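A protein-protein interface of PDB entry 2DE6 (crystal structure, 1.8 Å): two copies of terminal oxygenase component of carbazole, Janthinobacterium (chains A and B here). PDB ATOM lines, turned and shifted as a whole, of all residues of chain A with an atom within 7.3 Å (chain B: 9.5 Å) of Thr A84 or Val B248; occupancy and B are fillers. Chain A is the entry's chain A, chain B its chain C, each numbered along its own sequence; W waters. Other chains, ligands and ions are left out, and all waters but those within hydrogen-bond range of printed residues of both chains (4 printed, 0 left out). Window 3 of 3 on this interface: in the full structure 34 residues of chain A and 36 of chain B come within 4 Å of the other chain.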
ATOM      1  N   ASN A  56      15.419  36.429 -16.918  1.00  0.00           N
ATOM      2  CA  ASN A  56      15.840  35.118 -17.391  1.00  0.00           C
ATOM      3  C   ASN A  56      15.162  34.833 -18.718  1.00  0.00           C
ATOM      4  O   ASN A  56      14.106  35.388 -19.010  1.00  0.00           O
ATOM      5  CB  ASN A  56      15.463  34.039 -16.371  1.00  0.00           C
ATOM      6  CG  ASN A  56      16.166  32.719 -16.635  1.00  0.00           C
ATOM      7  OD1 ASN A  56      17.120  32.654 -17.417  1.00  0.00           O
ATOM      8  ND2 ASN A  56      15.707  31.662 -15.973  1.00  0.00           N
ATOM      9  N   ILE A  58      13.645  31.770 -20.876  1.00  0.00           N
ATOM     10  CA  ILE A  58      13.189  30.386 -20.776  1.00  0.00           C
ATOM     11  C   ILE A  58      12.414  30.043 -22.044  1.00  0.00           C
ATOM     12  O   ILE A  58      11.409  30.677 -22.358  1.00  0.00           O
ATOM     13  CB  ILE A  58      12.283  30.208 -19.538  1.00  0.00           C
ATOM     14  CG1 ILE A  58      13.044  30.662 -18.288  1.00  0.00           C
ATOM     15  CG2 ILE A  58      11.839  28.754 -19.405  1.00  0.00           C
ATOM     16  CD1 ILE A  58      12.234  30.606 -17.010  1.00  0.00           C
ATOM     17  N   GLU A  81      19.798  29.682  -7.643  1.00  0.00           N
ATOM     18  CA  GLU A  81      19.439  28.271  -7.603  1.00  0.00           C
ATOM     19  C   GLU A  81      18.168  28.027  -8.417  1.00  0.00           C
ATOM     20  O   GLU A  81      17.062  28.074  -7.884  1.00  0.00           O
ATOM     21  CB  GLU A  81      19.225  27.792  -6.155  1.00  0.00           C
ATOM     22  CG  GLU A  81      20.518  27.545  -5.373  1.00  0.00           C
ATOM     23  CD  GLU A  81      20.293  26.908  -4.001  1.00  0.00           C
ATOM     24  OE1 GLU A  81      19.294  26.178  -3.821  1.00  0.00           O
ATOM     25  OE2 GLU A  81      21.132  27.119  -3.102  1.00  0.00           O
ATOM     26  N   CYS A  82      18.326  27.804  -9.718  1.00  0.00           N
ATOM     27  CA  CYS A  82      17.183  27.504 -10.573  1.00  0.00           C
ATOM     28  C   CYS A  82      17.179  25.979 -10.649  1.00  0.00           C
ATOM     29  O   CYS A  82      17.896  25.379 -11.455  1.00  0.00           O
ATOM     30  CB  CYS A  82      17.361  28.123 -11.960  1.00  0.00           C
ATOM     31  SG  CYS A  82      17.179  29.938 -11.982  1.00  0.00           S
ATOM     32  N   LYS A  83      16.374  25.364  -9.791  1.00  0.00           N
ATOM     33  CA  LYS A  83      16.310  23.911  -9.699  1.00  0.00           C
ATOM     34  C   LYS A  83      15.423  23.217 -10.718  1.00  0.00           C
ATOM     35  O   LYS A  83      15.522  22.003 -10.904  1.00  0.00           O
ATOM     36  CB  LYS A  83      15.922  23.515  -8.276  1.00  0.00           C
ATOM     37  CG  LYS A  83      16.884  24.083  -7.249  1.00  0.00           C
ATOM     38  CD  LYS A  83      16.715  23.421  -5.894  1.00  0.00           C
ATOM     39  CE  LYS A  83      17.860  23.792  -4.967  1.00  0.00           C
ATOM     40  NZ  LYS A  83      19.198  23.483  -5.557  1.00  0.00           N
ATOM     41  N   THR A  84      14.536  23.976 -11.353  1.00  0.00           N
ATOM     42  CA  THR A  84      13.687  23.430 -12.408  1.00  0.00           C
ATOM     43  C   THR A  84      13.598  24.520 -13.456  1.00  0.00           C
ATOM     44  O   THR A  84      13.792  25.698 -13.158  1.00  0.00           O
ATOM     45  CB  THR A  84      12.261  23.041 -11.937  1.00  0.00           C
ATOM     46  OG1 THR A  84      11.466  24.214 -11.733  1.00  0.00           O
ATOM     47  CG2 THR A  84      12.326  22.217 -10.654  1.00  0.00           C
ATOM     48  N   LYS A  85      13.322  24.124 -14.687  1.00  0.00           N
ATOM     49  CA  LYS A  85      13.249  25.062 -15.793  1.00  0.00           C
ATOM     50  C   LYS A  85      12.390  26.300 -15.555  1.00  0.00           C
ATOM     51  O   LYS A  85      12.771  27.406 -15.938  1.00  0.00           O
ATOM     52  CB  LYS A  85      12.746  24.321 -17.035  1.00  0.00           C
ATOM     53  CG  LYS A  85      12.918  25.072 -18.335  1.00  0.00           C
ATOM     54  CD  LYS A  85      12.561  24.163 -19.503  1.00  0.00           C
ATOM     55  CE  LYS A  85      12.811  24.839 -20.832  1.00  0.00           C
ATOM     56  NZ  LYS A  85      12.490  23.921 -21.961  1.00  0.00           N
ATOM     57  N   SER A  86      11.246  26.120 -14.905  1.00  0.00           N
ATOM     58  CA  SER A  86      10.319  27.227 -14.689  1.00  0.00           C
ATOM     59  C   SER A  86      10.366  27.949 -13.348  1.00  0.00           C
ATOM     60  O   SER A  86       9.535  28.820 -13.099  1.00  0.00           O
ATOM     61  CB  SER A  86       8.893  26.731 -14.903  1.00  0.00           C
ATOM     62  OG  SER A  86       8.570  25.763 -13.920  1.00  0.00           O
ATOM     63  N   THR A  87      11.321  27.615 -12.491  1.00  0.00           N
ATOM     64  CA  THR A  87      11.368  28.261 -11.182  1.00  0.00           C
ATOM     65  C   THR A  87      12.750  28.706 -10.728  1.00  0.00           C
ATOM     66  O   THR A  87      13.764  28.396 -11.356  1.00  0.00           O
ATOM     67  CB  THR A  87      10.813  27.311 -10.086  1.00  0.00           C
ATOM     68  OG1 THR A  87      11.664  26.159  -9.976  1.00  0.00           O
ATOM     69  CG2 THR A  87       9.402  26.847 -10.437  1.00  0.00           C
ATOM     70  N   ILE A  88      12.765  29.479  -9.642  1.00  0.00           N
ATOM     71  CA  ILE A  88      14.004  29.905  -9.016  1.00  0.00           C
ATOM     72  C   ILE A  88      13.782  29.727  -7.515  1.00  0.00           C
ATOM     73  O   ILE A  88      12.728  30.087  -6.983  1.00  0.00           O
ATOM     74  CB  ILE A  88      14.397  31.371  -9.348  1.00  0.00           C
ATOM     75  CG1 ILE A  88      15.734  31.683  -8.665  1.00  0.00           C
ATOM     76  CG2 ILE A  88      13.304  32.342  -8.916  1.00  0.00           C
ATOM     77  CD1 ILE A  88      16.387  32.967  -9.117  1.00  0.00           C
ATOM     78  N   THR A  89      14.772  29.147  -6.847  1.00  0.00           N
ATOM     79  CA  THR A  89      14.691  28.876  -5.420  1.00  0.00           C
ATOM     80  C   THR A  89      15.647  29.761  -4.622  1.00  0.00           C
ATOM     81  O   THR A  89      16.838  29.811  -4.915  1.00  0.00           O
ATOM     82  CB  THR A  89      15.044  27.397  -5.145  1.00  0.00           C
ATOM     83  OG1 THR A  89      14.063  26.551  -5.763  1.00  0.00           O
ATOM     84  CG2 THR A  89      15.095  27.117  -3.646  1.00  0.00           C
ATOM     85  N   THR A  96      10.480  28.991  -3.203  1.00  0.00           N
ATOM     86  CA  THR A  96      10.575  28.829  -4.645  1.00  0.00           C
ATOM     87  C   THR A  96       9.481  29.570  -5.405  1.00  0.00           C
ATOM     88  O   THR A  96       8.300  29.472  -5.074  1.00  0.00           O
ATOM     89  CB  THR A  96      10.566  27.321  -4.978  1.00  0.00           C
ATOM     90  OG1 THR A  96      11.679  26.702  -4.314  1.00  0.00           O
ATOM     91  CG2 THR A  96      10.681  27.077  -6.477  1.00  0.00           C
ATOM     92  N   TYR A  97       9.896  30.302  -6.435  1.00  0.00           N
ATOM     93  CA  TYR A  97       8.984  31.118  -7.235  1.00  0.00           C
ATOM     94  C   TYR A  97       8.951  30.748  -8.711  1.00  0.00           C
ATOM     95  O   TYR A  97       9.961  30.334  -9.280  1.00  0.00           O
ATOM     96  CB  TYR A  97       9.407  32.584  -7.145  1.00  0.00           C
ATOM     97  CG  TYR A  97       9.629  33.090  -5.743  1.00  0.00           C
ATOM     98  CD1 TYR A  97       8.571  33.592  -4.992  1.00  0.00           C
ATOM     99  CD2 TYR A  97      10.902  33.087  -5.173  1.00  0.00           C
ATOM    100  CE1 TYR A  97       8.773  34.091  -3.705  1.00  0.00           C
ATOM    101  CE2 TYR A  97      11.117  33.579  -3.879  1.00  0.00           C
ATOM    102  CZ  TYR A  97      10.048  34.085  -3.159  1.00  0.00           C
ATOM    103  OH  TYR A  97      10.254  34.638  -1.914  1.00  0.00           O
ATOM    104  N   TRP A  99       8.841  31.820 -12.544  1.00  0.00           N
ATOM    105  CA  TRP A  99       9.229  32.980 -13.343  1.00  0.00           C
ATOM    106  C   TRP A  99       8.033  33.596 -14.062  1.00  0.00           C
ATOM    107  O   TRP A  99       7.967  34.810 -14.265  1.00  0.00           O
ATOM    108  CB  TRP A  99      10.274  32.588 -14.392  1.00  0.00           C
ATOM    109  CG  TRP A  99      11.636  32.359 -13.845  1.00  0.00           C
ATOM    110  CD1 TRP A  99      12.183  31.167 -13.465  1.00  0.00           C
ATOM    111  CD2 TRP A  99      12.633  33.357 -13.596  1.00  0.00           C
ATOM    112  NE1 TRP A  99      13.464  31.360 -12.994  1.00  0.00           N
ATOM    113  CE2 TRP A  99      13.763  32.696 -13.063  1.00  0.00           C
ATOM    114  CE3 TRP A  99      12.681  34.747 -13.772  1.00  0.00           C
ATOM    115  CZ2 TRP A  99      14.931  33.379 -12.702  1.00  0.00           C
ATOM    116  CZ3 TRP A  99      13.839  35.424 -13.415  1.00  0.00           C
ATOM    117  CH2 TRP A  99      14.949  34.740 -12.885  1.00  0.00           C
ATOM    118  N   CYS A 105       5.398  28.876  -5.254  1.00  0.00           N
ATOM    119  CA  CYS A 105       4.826  27.552  -5.502  1.00  0.00           C
ATOM    120  C   CYS A 105       5.323  26.405  -4.628  1.00  0.00           C
ATOM    121  O   CYS A 105       4.699  25.348  -4.578  1.00  0.00           O
ATOM    122  CB  CYS A 105       5.043  27.179  -6.968  1.00  0.00           C
ATOM    123  SG  CYS A 105       6.783  27.046  -7.433  1.00  0.00           S
ATOM    124  N   LEU A 108      11.119  24.425  -0.085  1.00  0.00           N
ATOM    125  CA  LEU A 108      11.831  23.190   0.224  1.00  0.00           C
ATOM    126  C   LEU A 108      12.047  22.910   1.704  1.00  0.00           C
ATOM    127  O   LEU A 108      12.035  21.751   2.118  1.00  0.00           O
ATOM    128  CB  LEU A 108      13.176  23.149  -0.511  1.00  0.00           C
ATOM    129  CG  LEU A 108      13.134  22.760  -1.992  1.00  0.00           C
ATOM    130  CD1 LEU A 108      12.292  23.735  -2.787  1.00  0.00           C
ATOM    131  CD2 LEU A 108      14.553  22.714  -2.529  1.00  0.00           C
ATOM    132  N   TYR B 185      19.328  24.979   5.514  1.00  0.00           N
ATOM    133  CA  TYR B 185      19.374  24.760   4.071  1.00  0.00           C
ATOM    134  C   TYR B 185      20.663  25.300   3.431  1.00  0.00           C
ATOM    135  O   TYR B 185      21.170  24.724   2.468  1.00  0.00           O
ATOM    136  CB  TYR B 185      18.169  25.440   3.411  1.00  0.00           C
ATOM    137  CG  TYR B 185      18.074  25.223   1.918  1.00  0.00           C
ATOM    138  CD1 TYR B 185      17.674  23.990   1.397  1.00  0.00           C
ATOM    139  CD2 TYR B 185      18.402  26.241   1.024  1.00  0.00           C
ATOM    140  CE1 TYR B 185      17.604  23.777   0.024  1.00  0.00           C
ATOM    141  CE2 TYR B 185      18.338  26.038  -0.356  1.00  0.00           C
ATOM    142  CZ  TYR B 185      17.939  24.804  -0.848  1.00  0.00           C
ATOM    143  OH  TYR B 185      17.890  24.588  -2.206  1.00  0.00           O
ATOM    144  N   LYS B 188      23.754  22.767   3.375  1.00  0.00           N
ATOM    145  CA  LYS B 188      23.672  21.479   2.696  1.00  0.00           C
ATOM    146  C   LYS B 188      24.925  21.020   1.952  1.00  0.00           C
ATOM    147  O   LYS B 188      25.157  19.816   1.834  1.00  0.00           O
ATOM    148  CB  LYS B 188      22.466  21.462   1.749  1.00  0.00           C
ATOM    149  CG  LYS B 188      22.496  22.510   0.651  1.00  0.00           C
ATOM    150  CD  LYS B 188      21.184  22.496  -0.125  1.00  0.00           C
ATOM    151  CE  LYS B 188      21.200  23.473  -1.289  1.00  0.00           C
ATOM    152  NZ  LYS B 188      21.409  24.883  -0.849  1.00  0.00           N
ATOM    153  N   ASP B 189      25.734  21.955   1.462  1.00  0.00           N
ATOM    154  CA  ASP B 189      26.948  21.582   0.737  1.00  0.00           C
ATOM    155  C   ASP B 189      28.244  21.818   1.517  1.00  0.00           C
ATOM    156  O   ASP B 189      29.330  21.705   0.956  1.00  0.00           O
ATOM    157  CB  ASP B 189      27.029  22.322  -0.604  1.00  0.00           C
ATOM    158  CG  ASP B 189      25.879  21.980  -1.540  1.00  0.00           C
ATOM    159  OD1 ASP B 189      25.541  20.783  -1.659  1.00  0.00           O
ATOM    160  OD2 ASP B 189      25.325  22.908  -2.168  1.00  0.00           O
ATOM    161  N   LEU B 202      17.209  19.182   5.303  1.00  0.00           N
ATOM    162  CA  LEU B 202      17.167  20.412   4.517  1.00  0.00           C
ATOM    163  C   LEU B 202      16.292  21.423   5.237  1.00  0.00           C
ATOM    164  O   LEU B 202      16.381  22.626   4.996  1.00  0.00           O
ATOM    165  CB  LEU B 202      16.565  20.143   3.138  1.00  0.00           C
ATOM    166  CG  LEU B 202      17.342  19.225   2.196  1.00  0.00           C
ATOM    167  CD1 LEU B 202      16.503  18.966   0.950  1.00  0.00           C
ATOM    168  CD2 LEU B 202      18.674  19.865   1.830  1.00  0.00           C
ATOM    169  N   PHE B 239      14.112  15.633   4.204  1.00  0.00           N
ATOM    170  CA  PHE B 239      15.308  15.068   3.591  1.00  0.00           C
ATOM    171  C   PHE B 239      15.187  15.025   2.074  1.00  0.00           C
ATOM    172  O   PHE B 239      16.189  14.908   1.370  1.00  0.00           O
ATOM    173  CB  PHE B 239      15.594  13.677   4.161  1.00  0.00           C
ATOM    174  CG  PHE B 239      16.335  13.713   5.464  1.00  0.00           C
ATOM    175  CD1 PHE B 239      17.718  13.869   5.484  1.00  0.00           C
ATOM    176  CD2 PHE B 239      15.648  13.662   6.671  1.00  0.00           C
ATOM    177  CE1 PHE B 239      18.408  13.976   6.693  1.00  0.00           C
ATOM    178  CE2 PHE B 239      16.328  13.767   7.883  1.00  0.00           C
ATOM    179  CZ  PHE B 239      17.707  13.926   7.893  1.00  0.00           C
ATOM    180  N   GLU B 240      13.957  15.125   1.575  1.00  0.00           N
ATOM    181  CA  GLU B 240      13.710  15.141   0.134  1.00  0.00           C
ATOM    182  C   GLU B 240      13.027  16.456  -0.232  1.00  0.00           C
ATOM    183  O   GLU B 240      11.834  16.631   0.017  1.00  0.00           O
ATOM    184  CB  GLU B 240      12.810  13.977  -0.299  1.00  0.00           C
ATOM    185  CG  GLU B 240      13.418  12.591  -0.129  1.00  0.00           C
ATOM    186  CD  GLU B 240      12.678  11.534  -0.935  1.00  0.00           C
ATOM    187  OE1 GLU B 240      11.435  11.455  -0.826  1.00  0.00           O
ATOM    188  OE2 GLU B 240      13.341  10.781  -1.681  1.00  0.00           O
ATOM    189  N   GLY B 241      13.788  17.381  -0.807  1.00  0.00           N
ATOM    190  CA  GLY B 241      13.229  18.664  -1.198  1.00  0.00           C
ATOM    191  C   GLY B 241      12.565  18.553  -2.556  1.00  0.00           C
ATOM    192  O   GLY B 241      13.185  18.097  -3.519  1.00  0.00           O
ATOM    193  N   THR B 242      11.312  18.990  -2.640  1.00  0.00           N
ATOM    194  CA  THR B 242      10.561  18.894  -3.883  1.00  0.00           C
ATOM    195  C   THR B 242      10.036  20.206  -4.472  1.00  0.00           C
ATOM    196  O   THR B 242       9.788  21.180  -3.762  1.00  0.00           O
ATOM    197  CB  THR B 242       9.336  17.964  -3.704  1.00  0.00           C
ATOM    198  OG1 THR B 242       8.489  18.490  -2.676  1.00  0.00           O
ATOM    199  CG2 THR B 242       9.772  16.552  -3.307  1.00  0.00           C
ATOM    200  N   ILE B 243       9.880  20.209  -5.789  1.00  0.00           N
ATOM    201  CA  ILE B 243       9.312  21.342  -6.504  1.00  0.00           C
ATOM    202  C   ILE B 243       8.277  20.701  -7.416  1.00  0.00           C
ATOM    203  O   ILE B 243       8.613  19.849  -8.245  1.00  0.00           O
ATOM    204  CB  ILE B 243      10.362  22.096  -7.342  1.00  0.00           C
ATOM    205  CG1 ILE B 243      11.362  22.790  -6.414  1.00  0.00           C
ATOM    206  CG2 ILE B 243       9.672  23.124  -8.236  1.00  0.00           C
ATOM    207  CD1 ILE B 243      12.432  23.604  -7.143  1.00  0.00           C
ATOM    208  N   GLY B 244       7.018  21.089  -7.254  1.00  0.00           N
ATOM    209  CA  GLY B 244       5.979  20.493  -8.070  1.00  0.00           C
ATOM    210  C   GLY B 244       5.853  19.007  -7.764  1.00  0.00           C
ATOM    211  O   GLY B 244       5.394  18.228  -8.603  1.00  0.00           O
ATOM    212  N   GLY B 245       6.275  18.616  -6.564  1.00  0.00           N
ATOM    213  CA  GLY B 245       6.193  17.222  -6.152  1.00  0.00           C
ATOM    214  C   GLY B 245       7.357  16.343  -6.576  1.00  0.00           C
ATOM    215  O   GLY B 245       7.416  15.166  -6.205  1.00  0.00           O
ATOM    216  N   GLU B 246       8.284  16.904  -7.347  1.00  0.00           N
ATOM    217  CA  GLU B 246       9.442  16.148  -7.818  1.00  0.00           C
ATOM    218  C   GLU B 246      10.676  16.462  -6.978  1.00  0.00           C
ATOM    219  O   GLU B 246      10.922  17.614  -6.632  1.00  0.00           O
ATOM    220  CB  GLU B 246       9.718  16.477  -9.283  1.00  0.00           C
ATOM    221  CG  GLU B 246       8.477  16.447 -10.152  1.00  0.00           C
ATOM    222  CD  GLU B 246       8.801  16.401 -11.631  1.00  0.00           C
ATOM    223  OE1 GLU B 246       9.849  16.953 -12.029  1.00  0.00           O
ATOM    224  OE2 GLU B 246       8.001  15.820 -12.391  1.00  0.00           O
ATOM    225  N   VAL B 247      11.456  15.434  -6.663  1.00  0.00           N
ATOM    226  CA  VAL B 247      12.650  15.614  -5.842  1.00  0.00           C
ATOM    227  C   VAL B 247      13.792  16.299  -6.594  1.00  0.00           C
ATOM    228  O   VAL B 247      14.278  15.786  -7.598  1.00  0.00           O
ATOM    229  CB  VAL B 247      13.146  14.254  -5.303  1.00  0.00           C
ATOM    230  CG1 VAL B 247      14.314  14.466  -4.352  1.00  0.00           C
ATOM    231  CG2 VAL B 247      12.007  13.536  -4.594  1.00  0.00           C
ATOM    232  N   VAL B 248      14.219  17.463  -6.107  1.00  0.00           N
ATOM    233  CA  VAL B 248      15.306  18.200  -6.751  1.00  0.00           C
ATOM    234  C   VAL B 248      16.556  18.272  -5.880  1.00  0.00           C
ATOM    235  O   VAL B 248      17.633  18.620  -6.360  1.00  0.00           O
ATOM    236  CB  VAL B 248      14.883  19.644  -7.116  1.00  0.00           C
ATOM    237  CG1 VAL B 248      13.773  19.619  -8.156  1.00  0.00           C
ATOM    238  CG2 VAL B 248      14.432  20.387  -5.866  1.00  0.00           C
ATOM    239  N   ARG B 249      16.411  17.952  -4.598  1.00  0.00           N
ATOM    240  CA  ARG B 249      17.548  17.972  -3.678  1.00  0.00           C
ATOM    241  C   ARG B 249      17.280  17.100  -2.457  1.00  0.00           C
ATOM    242  O   ARG B 249      16.151  17.009  -1.981  1.00  0.00           O
ATOM    243  CB  ARG B 249      17.842  19.403  -3.209  1.00  0.00           C
ATOM    244  CG  ARG B 249      18.934  19.484  -2.145  1.00  0.00           C
ATOM    245  CD  ARG B 249      20.319  19.263  -2.749  1.00  0.00           C
ATOM    246  NE  ARG B 249      21.314  18.924  -1.735  1.00  0.00           N
ATOM    247  CZ  ARG B 249      22.539  19.439  -1.691  1.00  0.00           C
ATOM    248  NH1 ARG B 249      22.922  20.325  -2.602  1.00  0.00           N
ATOM    249  NH2 ARG B 249      23.382  19.067  -0.738  1.00  0.00           N
ATOM    250  N   GLU B 250      18.326  16.458  -1.952  1.00  0.00           N
ATOM    251  CA  GLU B 250      18.188  15.628  -0.766  1.00  0.00           C
ATOM    252  C   GLU B 250      19.119  16.100   0.338  1.00  0.00           C
ATOM    253  O   GLU B 250      20.138  16.739   0.072  1.00  0.00           O
ATOM    254  CB  GLU B 250      18.492  14.165  -1.084  1.00  0.00           C
ATOM    255  CG  GLU B 250      17.399  13.467  -1.859  1.00  0.00           C
ATOM    256  CD  GLU B 250      17.610  11.970  -1.924  1.00  0.00           C
ATOM    257  OE1 GLU B 250      18.568  11.529  -2.593  1.00  0.00           O
ATOM    258  OE2 GLU B 250      16.822  11.235  -1.295  1.00  0.00           O
ATOM    259  N   GLY B 251      18.749  15.786   1.575  1.00  0.00           N
ATOM    260  CA  GLY B 251      19.564  16.149   2.718  1.00  0.00           C
ATOM    261  C   GLY B 251      20.704  15.155   2.843  1.00  0.00           C
ATOM    262  O   GLY B 251      20.900  14.324   1.954  1.00  0.00           O
HETATM  263  O   HOH W   1      21.363  21.734  -4.716  1.00  0.00           O
HETATM  264  O   HOH W   2      10.610  19.903   0.488  1.00  0.00           O
HETATM  265  O   HOH W   3      21.945  27.677  -0.445  1.00  0.00           O
HETATM  266  O   HOH W   4       5.065  23.866  -7.894  1.00  0.00           O
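OE1 of Glu A81 is in hydrogen-bond range of OH of Tyr B185 (2.7 Å).
The side-chain amino group of Lys B188 is in salt-bridge range of the side-chain carboxylate of Glu A81 (3.2 Å).
The side-chain sulfur (SG) of Cys A82 sits close to the backbone carbonyl oxygen (O) of Thr A87 (3.8 Å).
O of Thr A96 sits at hydrogen-bond distance from N of Cys A105 (3.0 Å).
The backbone carbonyl oxygen (O) of Thr A87 lies within hydrogen-bond range of the indole nitrogen (NE1) of Trp A99.
The backbone carbonyl oxygen of Gly B241 lies within hydrogen-bond range of the backbone NH of Val B248, at 2.9 Å.
The backbone carbonyl oxygen (O) of Lys B188 sits at hydrogen-bond distance from the guanidinium group (NH2) of Arg B249, 3.2 Å away.
O of Glu A81 lies within hydrogen-bond range of N of Thr A89 (2.7 Å).
Among the printed residues, pairs that only touch across the chains: Lys A83 with Tyr B185 (2.9 Å), Lys A83 with Ile B243 (3.7 Å), Lys A83 with Val B248 (3.8 Å), Thr A84 with Ile B243 (3.7 Å), Thr A84 with Val B248 (3.9 Å), Thr A87 with Ile B243 (3.9 Å), Thr A89 with Ile B243 (3.6 Å), Thr A96 with Ile B243 (3.9 Å), Leu A108 with Tyr B185 (3.8 Å), Leu A108 with Thr B242 (3.7 Å) and Leu A108 with Ile B243 (3.9 Å).
Of the printed residues of chain B, Thr A84 touches Ile B243 (3.7 Å) and Val B248 (3.9 Å).
Val B248 touches two residues of chain A.
No residue of chain B comes within 4 Å of Ser A86.
Of chain B, only Ile B243 (3.9 Å) comes within 4 Å of Thr A87.
Printed residues of chain A within 4 Å of Thr B242: Leu A108 (3.7 Å).
Of the printed residues of chain B, Leu A108 touches Tyr B185 (3.8 Å), Thr B242 (3.7 Å) and Ile B243 (3.9 Å).
Printed residues of chain B within 4 Å of Thr A89: Ile B243.
Of the printed residues of chain B, Glu A81 touches Tyr B185 and Lys B188.
Printed residues of chain B within 4 Å of Thr A96: Ile B243 (3.9 Å).
Ile A88 touches none of the printed residues of chain B.
Tyr A97 touches none of the printed residues of chain B.
The nearest residue of chain B that does not touch Thr A84 is Glu B246 (6.0 Å).
The nearest residue of chain A that does not touch Val B248 is Leu A108 (4.1 Å).
Hydrophobic or aromatic side chains of chain B that line the printed part of chain A: Tyr B185, Ile B243 and Val B248.
Among the printed residues, 13 pairs touch across the chains.
No position is printed for both chains.
Of the 13 pairs that touch across the chains among the printed residues, none has its exchanged pair printed and touching as well.
Water W3 lies within hydrogen-bond range of the side-chain carboxylate of Glu A81 and the side-chain amino group of Lys B188.
Water W2 lies within hydrogen-bond range of the backbone carbonyl oxygen of Leu A108 (2.8 Å) and the backbone NH of Thr B242 (3.3 Å).
Water W1 bridges the side-chain amino group (NZ) of Lys A83 and the guanidinium group (NH1) of Arg B249.
Water W4 lies within hydrogen-bond range of N of Gly B244 (3.5 Å) and SG of Cys A105 (3.6 Å).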
